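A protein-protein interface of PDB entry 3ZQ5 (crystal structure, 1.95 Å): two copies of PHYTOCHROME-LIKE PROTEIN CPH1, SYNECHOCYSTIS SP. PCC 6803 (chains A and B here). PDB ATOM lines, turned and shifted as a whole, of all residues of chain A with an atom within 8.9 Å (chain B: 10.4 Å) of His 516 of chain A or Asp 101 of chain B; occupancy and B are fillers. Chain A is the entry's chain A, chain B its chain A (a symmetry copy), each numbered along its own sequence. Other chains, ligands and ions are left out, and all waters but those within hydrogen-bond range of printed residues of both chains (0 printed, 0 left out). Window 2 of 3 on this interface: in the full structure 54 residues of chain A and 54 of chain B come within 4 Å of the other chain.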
ATOM      1  N   LEU A 509      14.839   1.251 -16.004  1.00  0.00           N
ATOM      2  CA  LEU A 509      15.909   1.399 -15.000  1.00  0.00           C
ATOM      3  C   LEU A 509      15.490   2.256 -13.803  1.00  0.00           C
ATOM      4  O   LEU A 509      15.796   1.929 -12.655  1.00  0.00           O
ATOM      5  CB  LEU A 509      17.171   1.994 -15.633  1.00  0.00           C
ATOM      6  CG  LEU A 509      18.126   0.977 -16.251  1.00  0.00           C
ATOM      7  CD1 LEU A 509      18.995   1.611 -17.342  1.00  0.00           C
ATOM      8  CD2 LEU A 509      18.988   0.343 -15.160  1.00  0.00           C
ATOM      9  N   ARG A 510      14.802   3.359 -14.084  1.00  0.00           N
ATOM     10  CA  ARG A 510      14.288   4.253 -13.041  1.00  0.00           C
ATOM     11  C   ARG A 510      13.242   3.566 -12.165  1.00  0.00           C
ATOM     12  O   ARG A 510      13.182   3.813 -10.961  1.00  0.00           O
ATOM     13  CB  ARG A 510      13.694   5.528 -13.661  1.00  0.00           C
ATOM     14  CG  ARG A 510      14.648   6.713 -13.689  1.00  0.00           C
ATOM     15  CD  ARG A 510      15.980   6.399 -14.392  1.00  0.00           C
ATOM     16  NE  ARG A 510      17.136   6.908 -13.648  1.00  0.00           N
ATOM     17  CZ  ARG A 510      18.394   6.903 -14.092  1.00  0.00           C
ATOM     18  NH1 ARG A 510      18.694   6.416 -15.296  1.00  0.00           N
ATOM     19  NH2 ARG A 510      19.364   7.398 -13.327  1.00  0.00           N
ATOM     20  N   GLN A 511      12.430   2.708 -12.779  1.00  0.00           N
ATOM     21  CA  GLN A 511      11.434   1.917 -12.059  1.00  0.00           C
ATOM     22  C   GLN A 511      12.075   0.791 -11.249  1.00  0.00           C
ATOM     23  O   GLN A 511      11.626   0.496 -10.144  1.00  0.00           O
ATOM     24  CB  GLN A 511      10.393   1.339 -13.027  1.00  0.00           C
ATOM     25  CG  GLN A 511       9.362   2.353 -13.512  1.00  0.00           C
ATOM     26  CD  GLN A 511       8.110   1.694 -14.061  1.00  0.00           C
ATOM     27  OE1 GLN A 511       7.096   1.590 -13.365  1.00  0.00           O
ATOM     28  NE2 GLN A 511       8.176   1.234 -15.310  1.00  0.00           N
ATOM     29  N   ALA A 512      13.114   0.165 -11.800  1.00  0.00           N
ATOM     30  CA  ALA A 512      13.905  -0.828 -11.061  1.00  0.00           C
ATOM     31  C   ALA A 512      14.665  -0.200  -9.888  1.00  0.00           C
ATOM     32  O   ALA A 512      14.808  -0.817  -8.831  1.00  0.00           O
ATOM     33  CB  ALA A 512      14.873  -1.542 -11.996  1.00  0.00           C
ATOM     34  N   GLU A 513      15.148   1.026 -10.084  1.00  0.00           N
ATOM     35  CA  GLU A 513      15.853   1.772  -9.039  1.00  0.00           C
ATOM     36  C   GLU A 513      14.914   2.254  -7.930  1.00  0.00           C
ATOM     37  O   GLU A 513      15.299   2.272  -6.760  1.00  0.00           O
ATOM     38  CB  GLU A 513      16.601   2.966  -9.646  1.00  0.00           C
ATOM     39  CG  GLU A 513      17.355   3.823  -8.632  1.00  0.00           C
ATOM     40  CD  GLU A 513      18.394   4.727  -9.272  1.00  0.00           C
ATOM     41  OE1 GLU A 513      18.162   5.200 -10.405  1.00  0.00           O
ATOM     42  OE2 GLU A 513      19.442   4.968  -8.636  1.00  0.00           O
ATOM     43  N   GLU A 514      13.697   2.653  -8.300  1.00  0.00           N
ATOM     44  CA  GLU A 514      12.702   3.129  -7.324  1.00  0.00           C
ATOM     45  C   GLU A 514      12.123   1.991  -6.478  1.00  0.00           C
ATOM     46  O   GLU A 514      11.820   2.188  -5.300  1.00  0.00           O
ATOM     47  CB  GLU A 514      11.558   3.897  -8.012  1.00  0.00           C
ATOM     48  CG  GLU A 514      11.569   5.408  -7.755  1.00  0.00           C
ATOM     49  CD  GLU A 514      11.084   5.781  -6.355  1.00  0.00           C
ATOM     50  OE1 GLU A 514      10.014   5.289  -5.936  1.00  0.00           O
ATOM     51  OE2 GLU A 514      11.771   6.576  -5.675  1.00  0.00           O
ATOM     52  N   HIS A 515      11.972   0.809  -7.077  1.00  0.00           N
ATOM     53  CA  HIS A 515      11.458  -0.362  -6.356  1.00  0.00           C
ATOM     54  C   HIS A 515      12.568  -1.121  -5.622  1.00  0.00           C
ATOM     55  O   HIS A 515      12.306  -2.138  -4.976  1.00  0.00           O
ATOM     56  CB  HIS A 515      10.705  -1.309  -7.306  1.00  0.00           C
ATOM     57  CG  HIS A 515       9.297  -1.591  -6.882  1.00  0.00           C
ATOM     58  ND1 HIS A 515       8.204  -1.171  -7.608  1.00  0.00           N
ATOM     59  CD2 HIS A 515       8.802  -2.241  -5.800  1.00  0.00           C
ATOM     60  CE1 HIS A 515       7.096  -1.554  -6.996  1.00  0.00           C
ATOM     61  NE2 HIS A 515       7.431  -2.204  -5.897  1.00  0.00           N
ATOM     62  N   HIS A 516      13.800  -0.628  -5.734  1.00  0.00           N
ATOM     63  CA  HIS A 516      14.900  -1.042  -4.862  1.00  0.00           C
ATOM     64  C   HIS A 516      15.047  -0.104  -3.652  1.00  0.00           C
ATOM     65  O   HIS A 516      15.055  -0.557  -2.505  1.00  0.00           O
ATOM     66  CB  HIS A 516      16.212  -1.083  -5.655  1.00  0.00           C
ATOM     67  CG  HIS A 516      17.428  -0.871  -4.811  1.00  0.00           C
ATOM     68  ND1 HIS A 516      17.951  -1.858  -4.004  1.00  0.00           N
ATOM     69  CD2 HIS A 516      18.207   0.221  -4.627  1.00  0.00           C
ATOM     70  CE1 HIS A 516      19.006  -1.387  -3.367  1.00  0.00           C
ATOM     71  NE2 HIS A 516      19.183  -0.128  -3.727  1.00  0.00           N
ATOM     72  N   HIS A 517      15.179   1.195  -3.928  1.00  0.00           N
ATOM     73  CA  HIS A 517      15.415   2.214  -2.893  1.00  0.00           C
ATOM     74  C   HIS A 517      14.204   2.351  -1.968  1.00  0.00           C
ATOM     75  O   HIS A 517      14.357   2.434  -0.746  1.00  0.00           O
ATOM     76  CB  HIS A 517      15.733   3.570  -3.543  1.00  0.00           C
ATOM     77  CG  HIS A 517      16.462   4.527  -2.647  1.00  0.00           C
ATOM     78  ND1 HIS A 517      17.648   5.129  -3.012  1.00  0.00           N
ATOM     79  CD2 HIS A 517      16.169   4.996  -1.409  1.00  0.00           C
ATOM     80  CE1 HIS A 517      18.056   5.923  -2.038  1.00  0.00           C
ATOM     81  NE2 HIS A 517      17.178   5.860  -1.054  1.00  0.00           N
ATOM     82  N   HIS A 518      13.010   2.375  -2.560  1.00  0.00           N
ATOM     83  CA  HIS A 518      11.757   2.473  -1.811  1.00  0.00           C
ATOM     84  C   HIS A 518      11.078   1.109  -1.712  1.00  0.00           C
ATOM     85  O   HIS A 518      11.497   0.249  -0.938  1.00  0.00           O
ATOM     86  CB  HIS A 518      10.816   3.476  -2.487  1.00  0.00           C
ATOM     87  CG  HIS A 518       9.634   3.855  -1.652  1.00  0.00           C
ATOM     88  ND1 HIS A 518       8.421   3.202  -1.737  1.00  0.00           N
ATOM     89  CD2 HIS A 518       9.478   4.817  -0.713  1.00  0.00           C
ATOM     90  CE1 HIS A 518       7.570   3.748  -0.887  1.00  0.00           C
ATOM     91  NE2 HIS A 518       8.186   4.729  -0.251  1.00  0.00           N
ATOM     92  N   TRP B  95      25.177  -0.176 -15.830  1.00  0.00           N
ATOM     93  CA  TRP B  95      25.105   0.128 -14.407  1.00  0.00           C
ATOM     94  C   TRP B  95      25.809  -0.923 -13.576  1.00  0.00           C
ATOM     95  O   TRP B  95      25.925  -2.079 -13.979  1.00  0.00           O
ATOM     96  CB  TRP B  95      23.647   0.318 -13.943  1.00  0.00           C
ATOM     97  CG  TRP B  95      22.784  -0.889 -14.142  1.00  0.00           C
ATOM     98  CD1 TRP B  95      22.445  -1.819 -13.199  1.00  0.00           C
ATOM     99  CD2 TRP B  95      22.164  -1.312 -15.363  1.00  0.00           C
ATOM    100  NE1 TRP B  95      21.650  -2.792 -13.759  1.00  0.00           N
ATOM    101  CE2 TRP B  95      21.465  -2.508 -15.086  1.00  0.00           C
ATOM    102  CE3 TRP B  95      22.137  -0.799 -16.667  1.00  0.00           C
ATOM    103  CZ2 TRP B  95      20.743  -3.193 -16.059  1.00  0.00           C
ATOM    104  CZ3 TRP B  95      21.426  -1.480 -17.631  1.00  0.00           C
ATOM    105  CH2 TRP B  95      20.735  -2.666 -17.323  1.00  0.00           C
ATOM    106  N   ALA B  96      26.324  -0.479 -12.436  1.00  0.00           N
ATOM    107  CA  ALA B  96      26.991  -1.335 -11.473  1.00  0.00           C
ATOM    108  C   ALA B  96      26.229  -1.223 -10.171  1.00  0.00           C
ATOM    109  O   ALA B  96      25.644  -0.179  -9.872  1.00  0.00           O
ATOM    110  CB  ALA B  96      28.438  -0.892 -11.276  1.00  0.00           C
ATOM    111  N   ARG B  97      26.245  -2.298  -9.394  1.00  0.00           N
ATOM    112  CA  ARG B  97      25.704  -2.273  -8.046  1.00  0.00           C
ATOM    113  C   ARG B  97      26.871  -2.004  -7.111  1.00  0.00           C
ATOM    114  O   ARG B  97      27.819  -2.784  -7.079  1.00  0.00           O
ATOM    115  CB  ARG B  97      25.029  -3.608  -7.712  1.00  0.00           C
ATOM    116  CG  ARG B  97      24.221  -4.243  -8.865  1.00  0.00           C
ATOM    117  CD  ARG B  97      23.211  -3.280  -9.485  1.00  0.00           C
ATOM    118  NE  ARG B  97      22.341  -2.664  -8.480  1.00  0.00           N
ATOM    119  CZ  ARG B  97      21.216  -3.200  -8.001  1.00  0.00           C
ATOM    120  NH1 ARG B  97      20.783  -4.387  -8.424  1.00  0.00           N
ATOM    121  NH2 ARG B  97      20.512  -2.538  -7.086  1.00  0.00           N
ATOM    122  N   VAL B  98      26.830  -0.896  -6.377  1.00  0.00           N
ATOM    123  CA  VAL B  98      27.954  -0.516  -5.512  1.00  0.00           C
ATOM    124  C   VAL B  98      27.617  -0.730  -4.034  1.00  0.00           C
ATOM    125  O   VAL B  98      26.465  -1.019  -3.694  1.00  0.00           O
ATOM    126  CB  VAL B  98      28.410   0.941  -5.746  1.00  0.00           C
ATOM    127  CG1 VAL B  98      28.658   1.187  -7.226  1.00  0.00           C
ATOM    128  CG2 VAL B  98      27.398   1.921  -5.191  1.00  0.00           C
ATOM    129  N   MET B  99      28.631  -0.588  -3.173  1.00  0.00           N
ATOM    130  CA  MET B  99      28.530  -0.845  -1.717  1.00  0.00           C
ATOM    131  C   MET B  99      27.590  -2.001  -1.336  1.00  0.00           C
ATOM    132  O   MET B  99      28.052  -3.071  -0.915  1.00  0.00           O
ATOM    133  CB  MET B  99      28.162   0.438  -0.936  1.00  0.00           C
ATOM    134  CG  MET B  99      27.493   1.553  -1.750  1.00  0.00           C
ATOM    135  SD  MET B  99      26.415   2.605  -0.755  1.00  0.00           S
ATOM    136  CE  MET B  99      25.025   1.504  -0.503  1.00  0.00           C
ATOM    137  N   GLY B 100      26.284  -1.771  -1.466  1.00  0.00           N
ATOM    138  CA  GLY B 100      25.283  -2.832  -1.330  1.00  0.00           C
ATOM    139  C   GLY B 100      23.951  -2.446  -1.949  1.00  0.00           C
ATOM    140  O   GLY B 100      23.484  -3.085  -2.896  1.00  0.00           O
ATOM    141  N   ASP B 101      23.351  -1.383  -1.416  1.00  0.00           N
ATOM    142  CA  ASP B 101      22.005  -0.957  -1.800  1.00  0.00           C
ATOM    143  C   ASP B 101      22.021   0.205  -2.821  1.00  0.00           C
ATOM    144  O   ASP B 101      21.251   1.162  -2.688  1.00  0.00           O
ATOM    145  CB  ASP B 101      21.202  -0.558  -0.542  1.00  0.00           C
ATOM    146  CG  ASP B 101      20.379  -1.709   0.028  1.00  0.00           C
ATOM    147  OD1 ASP B 101      20.918  -2.828   0.166  1.00  0.00           O
ATOM    148  OD2 ASP B 101      19.189  -1.488   0.346  1.00  0.00           O
ATOM    149  N   ASP B 102      22.870   0.120  -3.845  1.00  0.00           N
ATOM    150  CA  ASP B 102      23.098   1.266  -4.739  1.00  0.00           C
ATOM    151  C   ASP B 102      23.268   0.869  -6.212  1.00  0.00           C
ATOM    152  O   ASP B 102      24.066  -0.007  -6.538  1.00  0.00           O
ATOM    153  CB  ASP B 102      24.333   2.058  -4.285  1.00  0.00           C
ATOM    154  CG  ASP B 102      23.987   3.244  -3.385  1.00  0.00           C
ATOM    155  OD1 ASP B 102      23.136   3.102  -2.479  1.00  0.00           O
ATOM    156  OD2 ASP B 102      24.582   4.327  -3.584  1.00  0.00           O
ATOM    157  N   PHE B 103      22.495   1.522  -7.079  1.00  0.00           N
ATOM    158  CA  PHE B 103      22.808   1.637  -8.503  1.00  0.00           C
ATOM    159  C   PHE B 103      23.784   2.794  -8.727  1.00  0.00           C
ATOM    160  O   PHE B 103      23.617   3.876  -8.162  1.00  0.00           O
ATOM    161  CB  PHE B 103      21.543   1.950  -9.315  1.00  0.00           C
ATOM    162  CG  PHE B 103      20.642   0.768  -9.559  1.00  0.00           C
ATOM    163  CD1 PHE B 103      19.608   0.470  -8.678  1.00  0.00           C
ATOM    164  CD2 PHE B 103      20.788  -0.008 -10.702  1.00  0.00           C
ATOM    165  CE1 PHE B 103      18.757  -0.605  -8.913  1.00  0.00           C
ATOM    166  CE2 PHE B 103      19.941  -1.082 -10.947  1.00  0.00           C
ATOM    167  CZ  PHE B 103      18.925  -1.383 -10.050  1.00  0.00           C
ATOM    168  N   VAL B 104      24.787   2.577  -9.567  1.00  0.00           N
ATOM    169  CA  VAL B 104      25.446   3.677 -10.266  1.00  0.00           C
ATOM    170  C   VAL B 104      25.240   3.474 -11.764  1.00  0.00           C
ATOM    171  O   VAL B 104      25.602   2.432 -12.304  1.00  0.00           O
ATOM    172  CB  VAL B 104      26.949   3.753  -9.912  1.00  0.00           C
ATOM    173  CG1 VAL B 104      27.620   4.907 -10.634  1.00  0.00           C
ATOM    174  CG2 VAL B 104      27.118   3.908  -8.403  1.00  0.00           C
ATOM    175  N   ILE B 105      24.650   4.469 -12.425  1.00  0.00           N
ATOM    176  CA  ILE B 105      24.175   4.320 -13.806  1.00  0.00           C
ATOM    177  C   ILE B 105      25.002   5.218 -14.727  1.00  0.00           C
ATOM    178  O   ILE B 105      25.202   6.409 -14.445  1.00  0.00           O
ATOM    179  CB  ILE B 105      22.663   4.648 -13.921  1.00  0.00           C
ATOM    180  CG1 ILE B 105      21.851   3.697 -13.032  1.00  0.00           C
ATOM    181  CG2 ILE B 105      22.179   4.534 -15.371  1.00  0.00           C
ATOM    182  CD1 ILE B 105      20.365   4.013 -12.958  1.00  0.00           C
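The backbone carbonyl oxygen (O) of Asp 101 of chain B lies within hydrogen-bond range of a ring nitrogen (NE2) of His 516 of chain A (2.6 Å).
NE of Arg 510 of chain A lies within salt-bridge range of OE1 of Glu 513 of chain A, at 3.8 Å.
Among the printed residues, pairs that only touch across the chains: Arg 510 of chain A with Ile 105 of chain B (3.5 Å), Glu 513 of chain A with Ile 105 of chain B (3.6 Å), Leu 509 of chain A with Trp 95 of chain B (3.6 Å), His 516 of chain A with Asp 102 of chain B (3.7 Å), Glu 513 of chain A with Phe 103 of chain B (3.7 Å) and Ala 512 of chain A with Phe 103 of chain B (3.96 Å).
Asp 101 of chain B touches just one residue of chain A: His 516 (2.6 Å). No residue of chain A comes within 4 Å of Gly 100 of chain B. Asp 102 of chain B touches just one residue of chain A: His 516 (3.7 Å). Of the printed residues of chain A, Ile 105 of chain B touches Arg 510 and Glu 513. Printed residues of chain B within 4 Å of Arg 510 of chain A: Ile 105. Of the printed residues of chain B, Ala 512 of chain A touches Phe 103 (3.96 Å). The nearest residue of chain A that does not touch Asp 101 of chain B is His 517 of chain A (5.4 Å). The nearest printed residue of chain A that does not touch Ile 105 of chain B is Leu 509 of chain A (4.5 Å).
Printed residues of chain B that touch a printed residue of chain A: Trp 95, Asp 101, Asp 102, Phe 103 and Ile 105. Hydrophobic or aromatic side chains of chain B within 4 Å of the printed part of chain A: Trp 95, Phe 103 and Ile 105.
No position is printed for both chains. Of the 7 pairs that touch across the chains among the printed residues, none has its exchanged pair printed and touching as well.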
